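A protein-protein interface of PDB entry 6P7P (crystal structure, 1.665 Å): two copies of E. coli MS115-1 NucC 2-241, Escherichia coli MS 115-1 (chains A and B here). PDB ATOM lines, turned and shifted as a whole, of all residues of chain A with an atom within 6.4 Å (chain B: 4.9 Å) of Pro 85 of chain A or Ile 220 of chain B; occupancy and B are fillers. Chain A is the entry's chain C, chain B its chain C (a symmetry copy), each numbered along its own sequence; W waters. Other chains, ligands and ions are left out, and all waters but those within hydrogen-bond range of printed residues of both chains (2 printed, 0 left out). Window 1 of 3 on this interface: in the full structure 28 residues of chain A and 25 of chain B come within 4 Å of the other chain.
NH1 of Arg 81 of chain A sits at hydrogen-bond distance from O of Leu 52 of chain B, at 3.0 Å. O of Ile 232 of chain A is in hydrogen-bond range of NE2 of Gln 224 of chain B (3.1 Å).
OD2 of Asp 80 of chain A sits at hydrogen-bond distance from N of Tyr 83 of chain A (2.9 Å). The side-chain carboxylate (OD2) of Asp 80 of chain A is in hydrogen-bond range of the side-chain hydroxyl (OG) of Ser 84 of chain A (2.6 Å). The backbone carbonyl oxygen (O) of Ser 84 of chain A is in hydrogen-bond range of the guanidinium group (NH1) of Arg 81 of chain A (2.9 Å). N of Ile 87 of chain A sits at hydrogen-bond distance from O of Ile 95 of chain A, 3.0 Å away.
Tyr 51 of chain B touches Arg 81 of chain A. Pro 53 of chain B touches Arg 81 of chain A (CA to O, 3.5 Å). Pro 53 of chain B touches Tyr 83 of chain A. Pro 53 of chain B touches Ser 84 of chain A (CB to N, 3.7 Å). CB of Pro 85 of chain A touches O of Tyr 51 of chain B, 3.1 Å away. Pro 85 of chain A touches Ile 220 of chain B (CB to CD1, 3.9 Å). Phe 86 of chain A touches Tyr 51 of chain B. O of Ile 87 of chain A touches CE1 of Tyr 51 of chain B, at 3.9 Å. CG2 of Ile 234 of chain A touches O of Phe 217 of chain B, at 3.5 Å. Ile 234 of chain A touches Ala 221 of chain B.
Of the printed residues of chain B, Tyr 83 of chain A touches Pro 53. Printed residues of chain B within 4 Å of Ser 84 of chain A: Pro 53 (3.7 Å). Of chain B, only Tyr 51 (3.1 Å) and Ile 220 (3.9 Å) come within 4 Å of Pro 85 of chain A. Of the printed residues of chain B, Ile 87 of chain A touches Tyr 51 (3.9 Å). Of the printed residues of chain A, Tyr 51 of chain B touches Arg 81, Pro 85, Phe 86 and Ile 87. Arg 218 of chain B touches none of the printed residues of chain A. Ile 220 of chain B touches one residue of chain A. Of the printed residues of chain A, Ala 221 of chain B touches Ile 234 (3.97 Å). The nearest residue of chain B that does not touch Pro 85 of chain A is Pro 53 of chain B (4.1 Å). The nearest residue of chain A that does not touch Ile 220 of chain B is Ile 234 of chain A (4.1 Å). The nearest printed residue of chain A that does not touch Pro 53 of chain B is Pro 85 of chain A (4.1 Å).
Hydrophobic or aromatic side chains of chain B that line the printed part of chain A: Tyr 51, Pro 53, Phe 217, Ile 220 and Ala 221. Printed residues of chain A that touch a printed residue of chain B: Arg 81, Tyr 83, Ser 84, Pro 85, Phe 86, Ile 87, Ile 232 and Ile 234. Hydrophobic or aromatic side chains of chain A that line the printed part of chain B: Pro 85, Phe 86, Ile 232 and Ile 234. Among the printed residues, 12 pairs touch across the chains.
No position is printed for both chains. Of the 12 pairs that touch across the chains among the printed residues, none has its exchanged pair printed and touching as well.
Water W1 bridges the backbone carbonyl oxygen (O) of Tyr 83 of chain A (2.7 Å) and the side-chain amide nitrogen (NE2) of Gln 224 of chain B (3.0 Å). Water W2 lies within hydrogen-bond range of the side-chain amide oxygen (OE1) of Gln 224 of chain B, the backbone NH (N) of Ile 234 of chain A and the backbone carbonyl oxygen (O) of Ile 232 of chain A.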
ATOM      1  N   ASP A  80      26.582 -10.944 -18.284  1.00  0.00           N
ATOM      2  CA  ASP A  80      26.092 -11.256 -16.954  1.00  0.00           C
ATOM      3  C   ASP A  80      25.384 -12.600 -16.918  1.00  0.00           C
ATOM      4  O   ASP A  80      24.610 -12.935 -17.819  1.00  0.00           O
ATOM      5  CB  ASP A  80      25.097 -10.198 -16.483  1.00  0.00           C
ATOM      6  CG  ASP A  80      24.386 -10.615 -15.231  1.00  0.00           C
ATOM      7  OD1 ASP A  80      25.037 -10.561 -14.169  1.00  0.00           O
ATOM      8  OD2 ASP A  80      23.193 -11.002 -15.299  1.00  0.00           O
ATOM      9  N   ARG A  81      25.607 -13.322 -15.825  1.00  0.00           N
ATOM     10  CA  ARG A  81      24.758 -14.453 -15.453  1.00  0.00           C
ATOM     11  C   ARG A  81      24.191 -14.363 -14.041  1.00  0.00           C
ATOM     12  O   ARG A  81      23.370 -15.209 -13.682  1.00  0.00           O
ATOM     13  CB  ARG A  81      25.518 -15.783 -15.595  1.00  0.00           C
ATOM     14  CG  ARG A  81      25.460 -16.342 -17.019  1.00  0.00           C
ATOM     15  CD  ARG A  81      24.167 -17.094 -17.294  1.00  0.00           C
ATOM     16  NE  ARG A  81      24.109 -18.322 -16.518  1.00  0.00           N
ATOM     17  CZ  ARG A  81      23.074 -18.709 -15.788  1.00  0.00           C
ATOM     18  NH1 ARG A  81      21.979 -17.963 -15.736  1.00  0.00           N
ATOM     19  NH2 ARG A  81      23.128 -19.843 -15.126  1.00  0.00           N
ATOM     20  N   TYR A  83      22.147 -12.157 -12.889  1.00  0.00           N
ATOM     21  CA  TYR A  83      20.797 -11.619 -12.970  1.00  0.00           C
ATOM     22  C   TYR A  83      20.093 -11.986 -14.260  1.00  0.00           C
ATOM     23  O   TYR A  83      18.990 -11.502 -14.517  1.00  0.00           O
ATOM     24  CB  TYR A  83      20.819 -10.098 -12.858  1.00  0.00           C
ATOM     25  CG  TYR A  83      21.397  -9.646 -11.538  1.00  0.00           C
ATOM     26  CD1 TYR A  83      20.651  -9.719 -10.387  1.00  0.00           C
ATOM     27  CD2 TYR A  83      22.691  -9.177 -11.450  1.00  0.00           C
ATOM     28  CE1 TYR A  83      21.172  -9.326  -9.166  1.00  0.00           C
ATOM     29  CE2 TYR A  83      23.231  -8.794 -10.237  1.00  0.00           C
ATOM     30  CZ  TYR A  83      22.459  -8.861  -9.104  1.00  0.00           C
ATOM     31  OH  TYR A  83      22.982  -8.463  -7.900  1.00  0.00           O
ATOM     32  N   SER A  84      20.721 -12.816 -15.084  1.00  0.00           N
ATOM     33  CA  SER A  84      20.269 -13.052 -16.431  1.00  0.00           C
ATOM     34  C   SER A  84      20.248 -14.555 -16.682  1.00  0.00           C
ATOM     35  O   SER A  84      21.234 -15.233 -16.373  1.00  0.00           O
ATOM     36  CB  SER A  84      21.217 -12.420 -17.452  1.00  0.00           C
ATOM     37  OG  SER A  84      21.439 -11.025 -17.250  1.00  0.00           O
ATOM     38  N   PRO A  85      19.182 -15.089 -17.272  1.00  0.00           N
ATOM     39  CA  PRO A  85      19.191 -16.493 -17.690  1.00  0.00           C
ATOM     40  C   PRO A  85      19.969 -16.661 -18.987  1.00  0.00           C
ATOM     41  O   PRO A  85      20.157 -15.714 -19.748  1.00  0.00           O
ATOM     42  CB  PRO A  85      17.708 -16.781 -17.919  1.00  0.00           C
ATOM     43  CG  PRO A  85      17.181 -15.442 -18.453  1.00  0.00           C
ATOM     44  CD  PRO A  85      17.963 -14.381 -17.704  1.00  0.00           C
ATOM     45  N   PHE A  86      20.329 -17.909 -19.284  1.00  0.00           N
ATOM     46  CA  PHE A  86      20.576 -18.268 -20.676  1.00  0.00           C
ATOM     47  C   PHE A  86      19.245 -18.321 -21.419  1.00  0.00           C
ATOM     48  O   PHE A  86      18.208 -18.634 -20.843  1.00  0.00           O
ATOM     49  CB  PHE A  86      21.256 -19.640 -20.799  1.00  0.00           C
ATOM     50  CG  PHE A  86      22.710 -19.650 -20.404  1.00  0.00           C
ATOM     51  CD1 PHE A  86      23.634 -18.898 -21.104  1.00  0.00           C
ATOM     52  CD2 PHE A  86      23.150 -20.403 -19.325  1.00  0.00           C
ATOM     53  CE1 PHE A  86      24.953 -18.874 -20.715  1.00  0.00           C
ATOM     54  CE2 PHE A  86      24.485 -20.391 -18.940  1.00  0.00           C
ATOM     55  CZ  PHE A  86      25.383 -19.628 -19.648  1.00  0.00           C
ATOM     56  N   ILE A  87      19.274 -18.027 -22.717  1.00  0.00           N
ATOM     57  CA  ILE A  87      18.103 -18.310 -23.545  1.00  0.00           C
ATOM     58  C   ILE A  87      18.118 -19.771 -23.981  1.00  0.00           C
ATOM     59  O   ILE A  87      17.072 -20.413 -24.061  1.00  0.00           O
ATOM     60  CB  ILE A  87      18.063 -17.350 -24.756  1.00  0.00           C
ATOM     61  CG1 ILE A  87      17.805 -15.899 -24.307  1.00  0.00           C
ATOM     62  CG2 ILE A  87      17.004 -17.761 -25.789  1.00  0.00           C
ATOM     63  CD1 ILE A  87      16.628 -15.717 -23.391  1.00  0.00           C
ATOM     64  N   ILE A  95      23.415 -19.561 -25.983  1.00  0.00           N
ATOM     65  CA  ILE A  95      22.779 -18.403 -26.599  1.00  0.00           C
ATOM     66  C   ILE A  95      22.335 -17.504 -25.467  1.00  0.00           C
ATOM     67  O   ILE A  95      21.613 -17.948 -24.566  1.00  0.00           O
ATOM     68  CB  ILE A  95      21.599 -18.809 -27.497  1.00  0.00           C
ATOM     69  CG1 ILE A  95      22.115 -19.800 -28.555  1.00  0.00           C
ATOM     70  CG2 ILE A  95      20.964 -17.576 -28.154  1.00  0.00           C
ATOM     71  CD1 ILE A  95      21.058 -20.364 -29.450  1.00  0.00           C
ATOM     72  N   VAL A  96      22.826 -16.270 -25.463  1.00  0.00           N
ATOM     73  CA  VAL A  96      22.576 -15.361 -24.352  1.00  0.00           C
ATOM     74  C   VAL A  96      21.616 -14.260 -24.781  1.00  0.00           C
ATOM     75  O   VAL A  96      21.602 -13.861 -25.955  1.00  0.00           O
ATOM     76  CB  VAL A  96      23.889 -14.752 -23.803  1.00  0.00           C
ATOM     77  CG1 VAL A  96      24.802 -15.836 -23.274  1.00  0.00           C
ATOM     78  CG2 VAL A  96      24.587 -13.900 -24.860  1.00  0.00           C
ATOM     79  N   PRO A  97      20.813 -13.716 -23.864  1.00  0.00           N
ATOM     80  CA  PRO A  97      19.955 -12.589 -24.223  1.00  0.00           C
ATOM     81  C   PRO A  97      20.758 -11.308 -24.343  1.00  0.00           C
ATOM     82  O   PRO A  97      21.753 -11.100 -23.639  1.00  0.00           O
ATOM     83  CB  PRO A  97      18.972 -12.529 -23.051  1.00  0.00           C
ATOM     84  CG  PRO A  97      19.798 -12.988 -21.888  1.00  0.00           C
ATOM     85  CD  PRO A  97      20.657 -14.082 -22.445  1.00  0.00           C
ATOM     86  N   SER A 100      21.985  -9.279 -21.368  1.00  0.00           N
ATOM     87  CA  SER A 100      23.089  -9.727 -20.525  1.00  0.00           C
ATOM     88  C   SER A 100      24.456  -9.215 -20.972  1.00  0.00           C
ATOM     89  O   SER A 100      25.442  -9.400 -20.250  1.00  0.00           O
ATOM     90  CB  SER A 100      23.128 -11.249 -20.499  1.00  0.00           C
ATOM     91  OG  SER A 100      23.623 -11.759 -21.726  1.00  0.00           O
ATOM     92  N   ILE A 232      16.280  -7.645 -17.164  1.00  0.00           N
ATOM     93  CA  ILE A 232      15.628  -8.223 -18.329  1.00  0.00           C
ATOM     94  C   ILE A 232      14.140  -8.427 -18.092  1.00  0.00           C
ATOM     95  O   ILE A 232      13.708  -8.813 -16.998  1.00  0.00           O
ATOM     96  CB  ILE A 232      16.314  -9.554 -18.665  1.00  0.00           C
ATOM     97  CG1 ILE A 232      15.748 -10.144 -19.950  1.00  0.00           C
ATOM     98  CG2 ILE A 232      16.164 -10.548 -17.522  1.00  0.00           C
ATOM     99  CD1 ILE A 232      16.577 -11.322 -20.432  1.00  0.00           C
ATOM    100  N   ILE A 234      11.825 -10.979 -19.020  1.00  0.00           N
ATOM    101  CA  ILE A 234      11.784 -12.297 -19.629  1.00  0.00           C
ATOM    102  C   ILE A 234      10.427 -12.544 -20.286  1.00  0.00           C
ATOM    103  O   ILE A 234      10.330 -13.356 -21.216  1.00  0.00           O
ATOM    104  CB  ILE A 234      12.132 -13.397 -18.611  1.00  0.00           C
ATOM    105  CG1 ILE A 234      12.486 -14.687 -19.353  1.00  0.00           C
ATOM    106  CG2 ILE A 234      10.991 -13.646 -17.651  1.00  0.00           C
ATOM    107  CD1 ILE A 234      13.755 -14.592 -20.167  1.00  0.00           C
ATOM    108  N   TYR B  51      19.371 -22.666 -16.086  1.00  0.00           N
ATOM    109  CA  TYR B  51      18.772 -21.458 -16.646  1.00  0.00           C
ATOM    110  C   TYR B  51      18.512 -20.334 -15.655  1.00  0.00           C
ATOM    111  O   TYR B  51      18.501 -19.163 -16.082  1.00  0.00           O
ATOM    112  CB  TYR B  51      17.457 -21.818 -17.344  1.00  0.00           C
ATOM    113  CG  TYR B  51      17.713 -22.520 -18.675  1.00  0.00           C
ATOM    114  CD1 TYR B  51      18.138 -21.799 -19.756  1.00  0.00           C
ATOM    115  CD2 TYR B  51      17.576 -23.906 -18.816  1.00  0.00           C
ATOM    116  CE1 TYR B  51      18.411 -22.415 -20.960  1.00  0.00           C
ATOM    117  CE2 TYR B  51      17.847 -24.528 -20.027  1.00  0.00           C
ATOM    118  CZ  TYR B  51      18.257 -23.769 -21.094  1.00  0.00           C
ATOM    119  OH  TYR B  51      18.548 -24.347 -22.325  1.00  0.00           O
ATOM    120  N   LEU B  52      18.271 -20.609 -14.383  1.00  0.00           N
ATOM    121  CA  LEU B  52      18.053 -19.497 -13.467  1.00  0.00           C
ATOM    122  C   LEU B  52      19.307 -18.618 -13.396  1.00  0.00           C
ATOM    123  O   LEU B  52      20.441 -19.125 -13.443  1.00  0.00           O
ATOM    124  CB  LEU B  52      17.706 -19.985 -12.058  1.00  0.00           C
ATOM    125  CG  LEU B  52      16.305 -20.590 -11.834  1.00  0.00           C
ATOM    126  CD1 LEU B  52      16.132 -20.904 -10.340  1.00  0.00           C
ATOM    127  CD2 LEU B  52      15.194 -19.683 -12.344  1.00  0.00           C
ATOM    128  N   PRO B  53      19.126 -17.304 -13.224  1.00  0.00           N
ATOM    129  CA  PRO B  53      20.249 -16.441 -12.854  1.00  0.00           C
ATOM    130  C   PRO B  53      21.037 -17.038 -11.697  1.00  0.00           C
ATOM    131  O   PRO B  53      20.478 -17.674 -10.815  1.00  0.00           O
ATOM    132  CB  PRO B  53      19.564 -15.130 -12.455  1.00  0.00           C
ATOM    133  CG  PRO B  53      18.287 -15.093 -13.316  1.00  0.00           C
ATOM    134  CD  PRO B  53      17.845 -16.556 -13.313  1.00  0.00           C
ATOM    135  N   LEU B 216       9.326 -21.809 -16.447  1.00  0.00           N
ATOM    136  CA  LEU B 216      10.624 -21.227 -16.109  1.00  0.00           C
ATOM    137  C   LEU B 216      10.582 -19.711 -16.196  1.00  0.00           C
ATOM    138  O   LEU B 216      11.084 -19.012 -15.303  1.00  0.00           O
ATOM    139  CB  LEU B 216      11.682 -21.797 -17.044  1.00  0.00           C
ATOM    140  CG  LEU B 216      13.070 -21.195 -17.003  1.00  0.00           C
ATOM    141  CD1 LEU B 216      13.767 -21.499 -15.687  1.00  0.00           C
ATOM    142  CD2 LEU B 216      13.884 -21.744 -18.224  1.00  0.00           C
ATOM    143  N   PHE B 217       9.980 -19.177 -17.265  1.00  0.00           N
ATOM    144  CA  PHE B 217       9.908 -17.729 -17.402  1.00  0.00           C
ATOM    145  C   PHE B 217       9.020 -17.107 -16.334  1.00  0.00           C
ATOM    146  O   PHE B 217       9.334 -16.045 -15.791  1.00  0.00           O
ATOM    147  CB  PHE B 217       9.398 -17.354 -18.797  1.00  0.00           C
ATOM    148  CG  PHE B 217      10.375 -17.617 -19.922  1.00  0.00           C
ATOM    149  CD1 PHE B 217      11.602 -18.209 -19.698  1.00  0.00           C
ATOM    150  CD2 PHE B 217      10.041 -17.256 -21.219  1.00  0.00           C
ATOM    151  CE1 PHE B 217      12.484 -18.443 -20.723  1.00  0.00           C
ATOM    152  CE2 PHE B 217      10.926 -17.488 -22.251  1.00  0.00           C
ATOM    153  CZ  PHE B 217      12.137 -18.094 -21.999  1.00  0.00           C
ATOM    154  N   ARG B 218       7.888 -17.758 -16.014  1.00  0.00           N
ATOM    155  CA  ARG B 218       7.033 -17.257 -14.951  1.00  0.00           C
ATOM    156  C   ARG B 218       7.788 -17.202 -13.633  1.00  0.00           C
ATOM    157  O   ARG B 218       7.648 -16.241 -12.854  1.00  0.00           O
ATOM    158  CB  ARG B 218       5.788 -18.144 -14.840  1.00  0.00           C
ATOM    159  CG  ARG B 218       4.908 -17.860 -13.643  1.00  0.00           C
ATOM    160  CD  ARG B 218       3.928 -16.781 -13.921  1.00  0.00           C
ATOM    161  NE  ARG B 218       3.244 -16.348 -12.692  1.00  0.00           N
ATOM    162  CZ  ARG B 218       2.437 -15.295 -12.622  1.00  0.00           C
ATOM    163  NH1 ARG B 218       2.195 -14.580 -13.709  1.00  0.00           N
ATOM    164  NH2 ARG B 218       1.858 -14.975 -11.469  1.00  0.00           N
ATOM    165  N   LEU B 219       8.600 -18.217 -13.363  1.00  0.00           N
ATOM    166  CA  LEU B 219       9.359 -18.246 -12.123  1.00  0.00           C
ATOM    167  C   LEU B 219      10.391 -17.134 -12.100  1.00  0.00           C
ATOM    168  O   LEU B 219      10.546 -16.439 -11.089  1.00  0.00           O
ATOM    169  CB  LEU B 219      10.029 -19.606 -11.971  1.00  0.00           C
ATOM    170  CG  LEU B 219      10.905 -19.789 -10.736  1.00  0.00           C
ATOM    171  CD1 LEU B 219      10.144 -19.572  -9.449  1.00  0.00           C
ATOM    172  CD2 LEU B 219      11.566 -21.164 -10.774  1.00  0.00           C
ATOM    173  N   ILE B 220      11.115 -16.950 -13.198  1.00  0.00           N
ATOM    174  CA  ILE B 220      12.113 -15.882 -13.226  1.00  0.00           C
ATOM    175  C   ILE B 220      11.454 -14.525 -13.003  1.00  0.00           C
ATOM    176  O   ILE B 220      11.939 -13.690 -12.230  1.00  0.00           O
ATOM    177  CB  ILE B 220      12.902 -15.922 -14.549  1.00  0.00           C
ATOM    178  CG1 ILE B 220      13.789 -17.172 -14.603  1.00  0.00           C
ATOM    179  CG2 ILE B 220      13.725 -14.652 -14.699  1.00  0.00           C
ATOM    180  CD1 ILE B 220      14.403 -17.390 -15.980  1.00  0.00           C
ATOM    181  N   ALA B 221      10.347 -14.260 -13.702  1.00  0.00           N
ATOM    182  CA  ALA B 221       9.713 -12.958 -13.587  1.00  0.00           C
ATOM    183  C   ALA B 221       9.194 -12.727 -12.174  1.00  0.00           C
ATOM    184  O   ALA B 221       9.294 -11.620 -11.640  1.00  0.00           O
ATOM    185  CB  ALA B 221       8.578 -12.830 -14.604  1.00  0.00           C
ATOM    186  N   GLN B 222       8.591 -13.747 -11.562  1.00  0.00           N
ATOM    187  CA  GLN B 222       8.077 -13.560 -10.208  1.00  0.00           C
ATOM    188  C   GLN B 222       9.213 -13.426  -9.197  1.00  0.00           C
ATOM    189  O   GLN B 222       9.122 -12.623  -8.259  1.00  0.00           O
ATOM    190  CB  GLN B 222       7.164 -14.716  -9.825  1.00  0.00           C
ATOM    191  CG  GLN B 222       5.892 -14.750 -10.602  1.00  0.00           C
ATOM    192  CD  GLN B 222       5.056 -13.486 -10.393  1.00  0.00           C
ATOM    193  OE1 GLN B 222       4.829 -12.711 -11.330  1.00  0.00           O
ATOM    194  NE2 GLN B 222       4.622 -13.264  -9.155  1.00  0.00           N
ATOM    195  N   LEU B 223      10.290 -14.190  -9.362  1.00  0.00           N
ATOM    196  CA  LEU B 223      11.405 -14.062  -8.431  1.00  0.00           C
ATOM    197  C   LEU B 223      11.990 -12.654  -8.469  1.00  0.00           C
ATOM    198  O   LEU B 223      12.466 -12.145  -7.446  1.00  0.00           O
ATOM    199  CB  LEU B 223      12.474 -15.100  -8.754  1.00  0.00           C
ATOM    200  CG  LEU B 223      12.222 -16.548  -8.338  1.00  0.00           C
ATOM    201  CD1 LEU B 223      13.247 -17.484  -8.958  1.00  0.00           C
ATOM    202  CD2 LEU B 223      12.235 -16.633  -6.831  1.00  0.00           C
ATOM    203  N   GLN B 224      12.003 -12.008  -9.640  1.00  0.00           N
ATOM    204  CA  GLN B 224      12.571 -10.662  -9.694  1.00  0.00           C
ATOM    205  C   GLN B 224      11.937  -9.722  -8.671  1.00  0.00           C
ATOM    206  O   GLN B 224      12.613  -8.846  -8.123  1.00  0.00           O
ATOM    207  CB  GLN B 224      12.429 -10.071 -11.108  1.00  0.00           C
ATOM    208  CG  GLN B 224      13.469 -10.578 -12.068  1.00  0.00           C
ATOM    209  CD  GLN B 224      13.211 -10.146 -13.504  1.00  0.00           C
ATOM    210  OE1 GLN B 224      12.091  -9.816 -13.890  1.00  0.00           O
ATOM    211  NE2 GLN B 224      14.276 -10.112 -14.297  1.00  0.00           N
HETATM  212  O   HOH W   1      17.127 -10.086 -13.243  1.00  0.00           O
HETATM  213  O   HOH W   2      11.044 -10.560 -16.336  1.00  0.00           O
